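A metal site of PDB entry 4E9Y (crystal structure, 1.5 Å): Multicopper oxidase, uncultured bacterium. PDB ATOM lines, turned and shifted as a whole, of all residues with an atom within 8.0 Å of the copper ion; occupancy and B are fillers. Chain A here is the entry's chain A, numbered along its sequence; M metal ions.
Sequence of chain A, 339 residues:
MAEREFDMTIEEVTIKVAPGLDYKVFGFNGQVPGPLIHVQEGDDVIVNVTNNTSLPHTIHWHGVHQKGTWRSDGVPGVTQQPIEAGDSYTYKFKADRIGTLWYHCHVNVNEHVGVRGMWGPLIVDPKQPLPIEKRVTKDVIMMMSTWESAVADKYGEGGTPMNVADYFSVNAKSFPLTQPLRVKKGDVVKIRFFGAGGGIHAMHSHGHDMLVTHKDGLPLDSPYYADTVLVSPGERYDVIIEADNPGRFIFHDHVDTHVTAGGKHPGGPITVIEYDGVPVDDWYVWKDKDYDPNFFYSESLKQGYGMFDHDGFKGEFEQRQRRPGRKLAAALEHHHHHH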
ATOM      1  N   ILE A  10      19.097 -15.577  13.119  1.00  0.00           N
ATOM      2  CA  ILE A  10      20.416 -15.485  13.746  1.00  0.00           C
ATOM      3  C   ILE A  10      20.886 -14.063  13.431  1.00  0.00           C
ATOM      4  O   ILE A  10      20.893 -13.715  12.246  1.00  0.00           O
ATOM      5  CB  ILE A  10      21.402 -16.553  13.266  1.00  0.00           C
ATOM      6  CG1 ILE A  10      20.804 -17.961  13.190  1.00  0.00           C
ATOM      7  CG2 ILE A  10      22.649 -16.599  14.139  1.00  0.00           C
ATOM      8  CD1 ILE A  10      21.752 -18.963  12.534  1.00  0.00           C
ATOM      9  N   PHE A  26      26.367 -13.847  18.353  1.00  0.00           N
ATOM     10  CA  PHE A  26      25.478 -14.251  17.281  1.00  0.00           C
ATOM     11  C   PHE A  26      24.223 -14.775  17.983  1.00  0.00           C
ATOM     12  O   PHE A  26      24.101 -15.949  18.275  1.00  0.00           O
ATOM     13  CB  PHE A  26      26.106 -15.314  16.405  1.00  0.00           C
ATOM     14  CG  PHE A  26      27.322 -14.894  15.611  1.00  0.00           C
ATOM     15  CD1 PHE A  26      27.256 -13.840  14.711  1.00  0.00           C
ATOM     16  CD2 PHE A  26      28.532 -15.559  15.765  1.00  0.00           C
ATOM     17  CE1 PHE A  26      28.362 -13.449  13.979  1.00  0.00           C
ATOM     18  CE2 PHE A  26      29.645 -15.191  15.034  1.00  0.00           C
ATOM     19  CZ  PHE A  26      29.558 -14.127  14.136  1.00  0.00           C
ATOM     20  N   PHE A  28      20.489 -15.991  18.645  1.00  0.00           N
ATOM     21  CA  PHE A  28      19.237 -16.471  18.084  1.00  0.00           C
ATOM     22  C   PHE A  28      18.147 -15.463  18.428  1.00  0.00           C
ATOM     23  O   PHE A  28      17.995 -15.110  19.605  1.00  0.00           O
ATOM     24  CB  PHE A  28      18.925 -17.858  18.649  1.00  0.00           C
ATOM     25  CG  PHE A  28      19.906 -18.893  18.106  1.00  0.00           C
ATOM     26  CD1 PHE A  28      19.942 -19.171  16.748  1.00  0.00           C
ATOM     27  CD2 PHE A  28      20.779 -19.566  18.946  1.00  0.00           C
ATOM     28  CE1 PHE A  28      20.822 -20.105  16.228  1.00  0.00           C
ATOM     29  CE2 PHE A  28      21.630 -20.526  18.433  1.00  0.00           C
ATOM     30  CZ  PHE A  28      21.638 -20.818  17.077  1.00  0.00           C
ATOM     31  N   ASN A  51      19.611 -16.984   8.542  1.00  0.00           N
ATOM     32  CA  ASN A  51      20.891 -16.482   8.973  1.00  0.00           C
ATOM     33  C   ASN A  51      21.105 -15.023   8.547  1.00  0.00           C
ATOM     34  O   ASN A  51      21.539 -14.796   7.411  1.00  0.00           O
ATOM     35  CB  ASN A  51      22.012 -17.353   8.376  1.00  0.00           C
ATOM     36  CG  ASN A  51      23.381 -16.923   8.847  1.00  0.00           C
ATOM     37  OD1 ASN A  51      23.540 -15.935   9.578  1.00  0.00           O
ATOM     38  ND2 ASN A  51      24.391 -17.687   8.414  1.00  0.00           N
ATOM     39  N   THR A  53      23.402 -13.077   9.678  1.00  0.00           N
ATOM     40  CA  THR A  53      24.750 -12.646  10.065  1.00  0.00           C
ATOM     41  C   THR A  53      25.706 -12.808   8.888  1.00  0.00           C
ATOM     42  O   THR A  53      25.327 -13.274   7.816  1.00  0.00           O
ATOM     43  CB  THR A  53      25.312 -13.469  11.249  1.00  0.00           C
ATOM     44  OG1 THR A  53      25.817 -14.737  10.766  1.00  0.00           O
ATOM     45  CG2 THR A  53      24.216 -13.779  12.248  1.00  0.00           C
ATOM     46  N   LEU A  55      28.330 -14.822   8.800  1.00  0.00           N
ATOM     47  CA  LEU A  55      29.097 -16.071   8.808  1.00  0.00           C
ATOM     48  C   LEU A  55      28.153 -17.250   8.781  1.00  0.00           C
ATOM     49  O   LEU A  55      26.973 -17.100   9.111  1.00  0.00           O
ATOM     50  CB  LEU A  55      29.960 -16.190  10.063  1.00  0.00           C
ATOM     51  CG  LEU A  55      31.113 -15.207  10.257  1.00  0.00           C
ATOM     52  CD1 LEU A  55      31.751 -15.381  11.622  1.00  0.00           C
ATOM     53  CD2 LEU A  55      32.126 -15.402   9.129  1.00  0.00           C
ATOM     54  N   PRO A  56      28.643 -18.425   8.408  1.00  0.00           N
ATOM     55  CA  PRO A  56      27.793 -19.603   8.376  1.00  0.00           C
ATOM     56  C   PRO A  56      27.555 -20.161   9.790  1.00  0.00           C
ATOM     57  O   PRO A  56      28.413 -20.004  10.673  1.00  0.00           O
ATOM     58  CB  PRO A  56      28.579 -20.634   7.581  1.00  0.00           C
ATOM     59  CG  PRO A  56      29.873 -20.010   7.221  1.00  0.00           C
ATOM     60  CD  PRO A  56      30.006 -18.720   7.957  1.00  0.00           C
ATOM     61  N   HIS A  57      26.376 -20.748   9.927  1.00  0.00           N
ATOM     62  CA  HIS A  57      25.940 -21.383  11.162  1.00  0.00           C
ATOM     63  C   HIS A  57      25.139 -22.649  10.855  1.00  0.00           C
ATOM     64  O   HIS A  57      24.772 -22.935   9.719  1.00  0.00           O
ATOM     65  CB  HIS A  57      25.053 -20.433  11.978  1.00  0.00           C
ATOM     66  CG  HIS A  57      25.708 -19.125  12.294  1.00  0.00           C
ATOM     67  ND1 HIS A  57      26.703 -18.971  13.215  1.00  0.00           N
ATOM     68  CD2 HIS A  57      25.541 -17.888  11.748  1.00  0.00           C
ATOM     69  CE1 HIS A  57      27.124 -17.723  13.269  1.00  0.00           C
ATOM     70  NE2 HIS A  57      26.399 -17.036  12.359  1.00  0.00           N
ATOM     71  N   THR A  58      24.766 -23.415  11.872  1.00  0.00           N
ATOM     72  CA  THR A  58      23.726 -24.420  11.822  1.00  0.00           C
ATOM     73  C   THR A  58      23.015 -24.380  13.194  1.00  0.00           C
ATOM     74  O   THR A  58      23.437 -23.610  14.069  1.00  0.00           O
ATOM     75  CB  THR A  58      24.220 -25.857  11.656  1.00  0.00           C
ATOM     76  OG1 THR A  58      25.119 -26.103  12.766  1.00  0.00           O
ATOM     77  CG2 THR A  58      25.042 -26.108  10.396  1.00  0.00           C
ATOM     78  N   ILE A  59      22.013 -25.206  13.391  1.00  0.00           N
ATOM     79  CA  ILE A  59      21.521 -25.455  14.753  1.00  0.00           C
ATOM     80  C   ILE A  59      21.500 -26.969  14.982  1.00  0.00           C
ATOM     81  O   ILE A  59      20.840 -27.699  14.235  1.00  0.00           O
ATOM     82  CB  ILE A  59      20.139 -24.867  15.046  1.00  0.00           C
ATOM     83  CG1 ILE A  59      20.023 -23.383  14.659  1.00  0.00           C
ATOM     84  CG2 ILE A  59      19.717 -25.061  16.496  1.00  0.00           C
ATOM     85  CD1 ILE A  59      18.667 -22.809  15.054  1.00  0.00           C
ATOM     86  N   ILE A  83      24.555 -23.318   7.023  1.00  0.00           N
ATOM     87  CA  ILE A  83      23.626 -22.290   6.575  1.00  0.00           C
ATOM     88  C   ILE A  83      24.441 -21.046   6.331  1.00  0.00           C
ATOM     89  O   ILE A  83      24.955 -20.368   7.234  1.00  0.00           O
ATOM     90  CB  ILE A  83      22.539 -22.051   7.623  1.00  0.00           C
ATOM     91  CG1 ILE A  83      21.818 -23.335   8.084  1.00  0.00           C
ATOM     92  CG2 ILE A  83      21.538 -21.019   7.125  1.00  0.00           C
ATOM     93  CD1 ILE A  83      20.926 -23.128   9.296  1.00  0.00           C
ATOM     94  N   HIS A 104      22.129 -25.405  19.896  1.00  0.00           N
ATOM     95  CA  HIS A 104      23.268 -24.542  19.774  1.00  0.00           C
ATOM     96  C   HIS A 104      23.860 -24.659  18.361  1.00  0.00           C
ATOM     97  O   HIS A 104      23.621 -25.666  17.681  1.00  0.00           O
ATOM     98  CB  HIS A 104      24.384 -24.812  20.789  1.00  0.00           C
ATOM     99  CG  HIS A 104      24.916 -26.219  20.819  1.00  0.00           C
ATOM    100  ND1 HIS A 104      25.859 -26.744  19.964  1.00  0.00           N
ATOM    101  CD2 HIS A 104      24.602 -27.235  21.665  1.00  0.00           C
ATOM    102  CE1 HIS A 104      26.096 -28.021  20.271  1.00  0.00           C
ATOM    103  NE2 HIS A 104      25.354 -28.332  21.302  1.00  0.00           N
ATOM    104  N   CYS A 105      24.626 -23.656  17.989  1.00  0.00           N
ATOM    105  CA  CYS A 105      25.222 -23.789  16.641  1.00  0.00           C
ATOM    106  C   CYS A 105      26.205 -24.939  16.662  1.00  0.00           C
ATOM    107  O   CYS A 105      26.755 -25.252  17.729  1.00  0.00           O
ATOM    108  CB  CYS A 105      25.902 -22.473  16.292  1.00  0.00           C
ATOM    109  SG  CYS A 105      26.734 -22.519  14.674  1.00  0.00           S
ATOM    110  N   HIS A 106      26.502 -25.572  15.537  1.00  0.00           N
ATOM    111  CA  HIS A 106      27.514 -26.621  15.492  1.00  0.00           C
ATOM    112  C   HIS A 106      28.604 -26.316  14.450  1.00  0.00           C
ATOM    113  O   HIS A 106      29.292 -27.245  14.004  1.00  0.00           O
ATOM    114  CB  HIS A 106      26.887 -27.983  15.197  1.00  0.00           C
ATOM    115  CG  HIS A 106      27.508 -29.070  16.001  1.00  0.00           C
ATOM    116  ND1 HIS A 106      28.781 -29.546  15.735  1.00  0.00           N
ATOM    117  CD2 HIS A 106      27.041 -29.783  17.053  1.00  0.00           C
ATOM    118  CE1 HIS A 106      29.071 -30.493  16.601  1.00  0.00           C
ATOM    119  NE2 HIS A 106      28.038 -30.669  17.411  1.00  0.00           N
ATOM    120  N   VAL A 107      28.765 -25.057  14.078  1.00  0.00           N
ATOM    121  CA  VAL A 107      29.836 -24.569  13.236  1.00  0.00           C
ATOM    122  C   VAL A 107      30.844 -23.800  14.129  1.00  0.00           C
ATOM    123  O   VAL A 107      30.346 -22.997  14.919  1.00  0.00           O
ATOM    124  CB  VAL A 107      29.334 -23.580  12.174  1.00  0.00           C
ATOM    125  CG1 VAL A 107      30.531 -23.074  11.346  1.00  0.00           C
ATOM    126  CG2 VAL A 107      28.275 -24.165  11.249  1.00  0.00           C
ATOM    127  N   ASN A 108      32.139 -24.025  13.981  1.00  0.00           N
ATOM    128  CA  ASN A 108      33.147 -23.233  14.694  1.00  0.00           C
ATOM    129  C   ASN A 108      32.795 -23.148  16.178  1.00  0.00           C
ATOM    130  O   ASN A 108      32.844 -22.094  16.823  1.00  0.00           O
ATOM    131  CB  ASN A 108      33.218 -21.844  14.061  1.00  0.00           C
ATOM    132  CG  ASN A 108      33.967 -21.714  12.737  1.00  0.00           C
ATOM    133  OD1 ASN A 108      34.749 -22.559  12.312  1.00  0.00           O
ATOM    134  ND2 ASN A 108      33.754 -20.598  12.016  1.00  0.00           N
ATOM    135  N   VAL A 109      32.387 -24.301  16.712  1.00  0.00           N
ATOM    136  CA  VAL A 109      31.764 -24.325  18.042  1.00  0.00           C
ATOM    137  C   VAL A 109      32.618 -23.761  19.165  1.00  0.00           C
ATOM    138  O   VAL A 109      32.048 -23.172  20.092  1.00  0.00           O
ATOM    139  CB  VAL A 109      31.290 -25.752  18.427  1.00  0.00           C
ATOM    140  CG1 VAL A 109      30.413 -26.288  17.309  1.00  0.00           C
ATOM    141  CG2 VAL A 109      32.431 -26.711  18.711  1.00  0.00           C
ATOM    142  N   GLU A 111      34.272 -21.253  19.214  1.00  0.00           N
ATOM    143  CA  GLU A 111      34.026 -19.820  19.314  1.00  0.00           C
ATOM    144  C   GLU A 111      32.537 -19.534  19.407  1.00  0.00           C
ATOM    145  O   GLU A 111      32.125 -18.765  20.298  1.00  0.00           O
ATOM    146  CB  GLU A 111      34.592 -19.067  18.091  1.00  0.00           C
ATOM    147  CG  GLU A 111      34.474 -17.554  18.221  1.00  0.00           C
ATOM    148  CD  GLU A 111      34.580 -16.788  16.917  1.00  0.00           C
ATOM    149  OE1 GLU A 111      35.086 -17.367  15.940  1.00  0.00           O
ATOM    150  OE2 GLU A 111      34.139 -15.612  16.904  1.00  0.00           O
ATOM    151  N   HIS A 112      31.748 -20.123  18.500  1.00  0.00           N
ATOM    152  CA  HIS A 112      30.326 -19.731  18.429  1.00  0.00           C
ATOM    153  C   HIS A 112      29.572 -20.148  19.679  1.00  0.00           C
ATOM    154  O   HIS A 112      28.730 -19.396  20.183  1.00  0.00           O
ATOM    155  CB  HIS A 112      29.682 -20.307  17.171  1.00  0.00           C
ATOM    156  CG  HIS A 112      30.156 -19.630  15.911  1.00  0.00           C
ATOM    157  ND1 HIS A 112      29.447 -19.765  14.730  1.00  0.00           N
ATOM    158  CD2 HIS A 112      31.225 -18.850  15.659  1.00  0.00           C
ATOM    159  CE1 HIS A 112      30.083 -19.083  13.791  1.00  0.00           C
ATOM    160  NE2 HIS A 112      31.166 -18.520  14.314  1.00  0.00           N
ATOM    161  N   VAL A 113      29.860 -21.365  20.181  1.00  0.00           N
ATOM    162  CA  VAL A 113      29.155 -21.785  21.396  1.00  0.00           C
ATOM    163  C   VAL A 113      29.959 -21.286  22.575  1.00  0.00           C
ATOM    164  O   VAL A 113      29.421 -20.869  23.604  1.00  0.00           O
ATOM    165  CB  VAL A 113      28.951 -23.304  21.435  1.00  0.00           C
ATOM    166  CG1 VAL A 113      28.276 -23.735  22.729  1.00  0.00           C
ATOM    167  CG2 VAL A 113      28.121 -23.723  20.223  1.00  0.00           C
ATOM    168  N   ARG A 116      30.126 -16.855  21.680  1.00  0.00           N
ATOM    169  CA  ARG A 116      29.247 -15.984  20.878  1.00  0.00           C
ATOM    170  C   ARG A 116      27.762 -16.231  21.187  1.00  0.00           C
ATOM    171  O   ARG A 116      26.879 -15.788  20.458  1.00  0.00           O
ATOM    172  CB  ARG A 116      29.482 -16.170  19.387  1.00  0.00           C
ATOM    173  CG  ARG A 116      30.870 -15.777  18.898  1.00  0.00           C
ATOM    174  CD  ARG A 116      31.249 -14.332  19.164  1.00  0.00           C
ATOM    175  NE  ARG A 116      32.713 -14.186  19.001  1.00  0.00           N
ATOM    176  CZ  ARG A 116      33.454 -13.202  19.469  1.00  0.00           C
ATOM    177  NH1 ARG A 116      32.967 -12.157  20.143  1.00  0.00           N
ATOM    178  NH2 ARG A 116      34.770 -13.260  19.244  1.00  0.00           N
ATOM    179  N   MET A 118      25.637 -18.681  21.068  1.00  0.00           N
ATOM    180  CA  MET A 118      24.754 -19.396  20.149  1.00  0.00           C
ATOM    181  C   MET A 118      24.119 -20.624  20.768  1.00  0.00           C
ATOM    182  O   MET A 118      24.388 -21.772  20.432  1.00  0.00           O
ATOM    183  CB  MET A 118      25.566 -19.771  18.891  1.00  0.00           C
ATOM    184  CG  MET A 118      26.124 -18.508  18.207  1.00  0.00           C
ATOM    185  SD  MET A 118      26.384 -18.850  16.425  1.00  0.00           S
ATOM    186  CE  MET A 118      24.682 -18.873  15.841  1.00  0.00           C
HETATM  187 CU    CU M   1      27.578 -20.382  14.495  1.00  0.00          CU
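A ring nitrogen (ND1) of His 112 lies close to the backbone carbonyl oxygen (O) of Val 107 (3.4 Å).
A ring nitrogen (NE2) of His 57 sits close to the backbone carbonyl oxygen of Leu 55, 3.3 Å away.
The side-chain hydroxyl (OG1) of Thr 53 lies within hydrogen-bond range of a ring nitrogen (NE2) of His 57, 2.9 Å away.
The backbone NH of Ile 83 sits at hydrogen-bond distance from the backbone carbonyl oxygen of His 57, 2.7 Å away.
SG of Cys 105 sits close to N of Val 107, 3.3 Å away.
The side-chain sulfur of Cys 105 lies close to the backbone carbonyl oxygen of Thr 58, at 3.5 Å.
The copper ion is bound by a ring nitrogen (ND1) of His 112 (2.0 Å), a ring nitrogen (ND1) of His 57 (2.1 Å), the side-chain sulfur (SG) of Cys 105 (2.3 Å) and the side-chain sulfur (SD) of Met 118 (2.7 Å).
The copper ion has four donor atoms within binding distance.
Pro 56 touches the copper ion.
Val 107 touches the copper ion (O to CU, 3.8 Å).
Six residues have an atom within 4 Å of the copper ion: Pro 56, His 57, Cys 105, Val 107, His 112 and Met 118.
The nearest printed residue that does not touch the copper ion is Thr 58 (4.9 Å).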
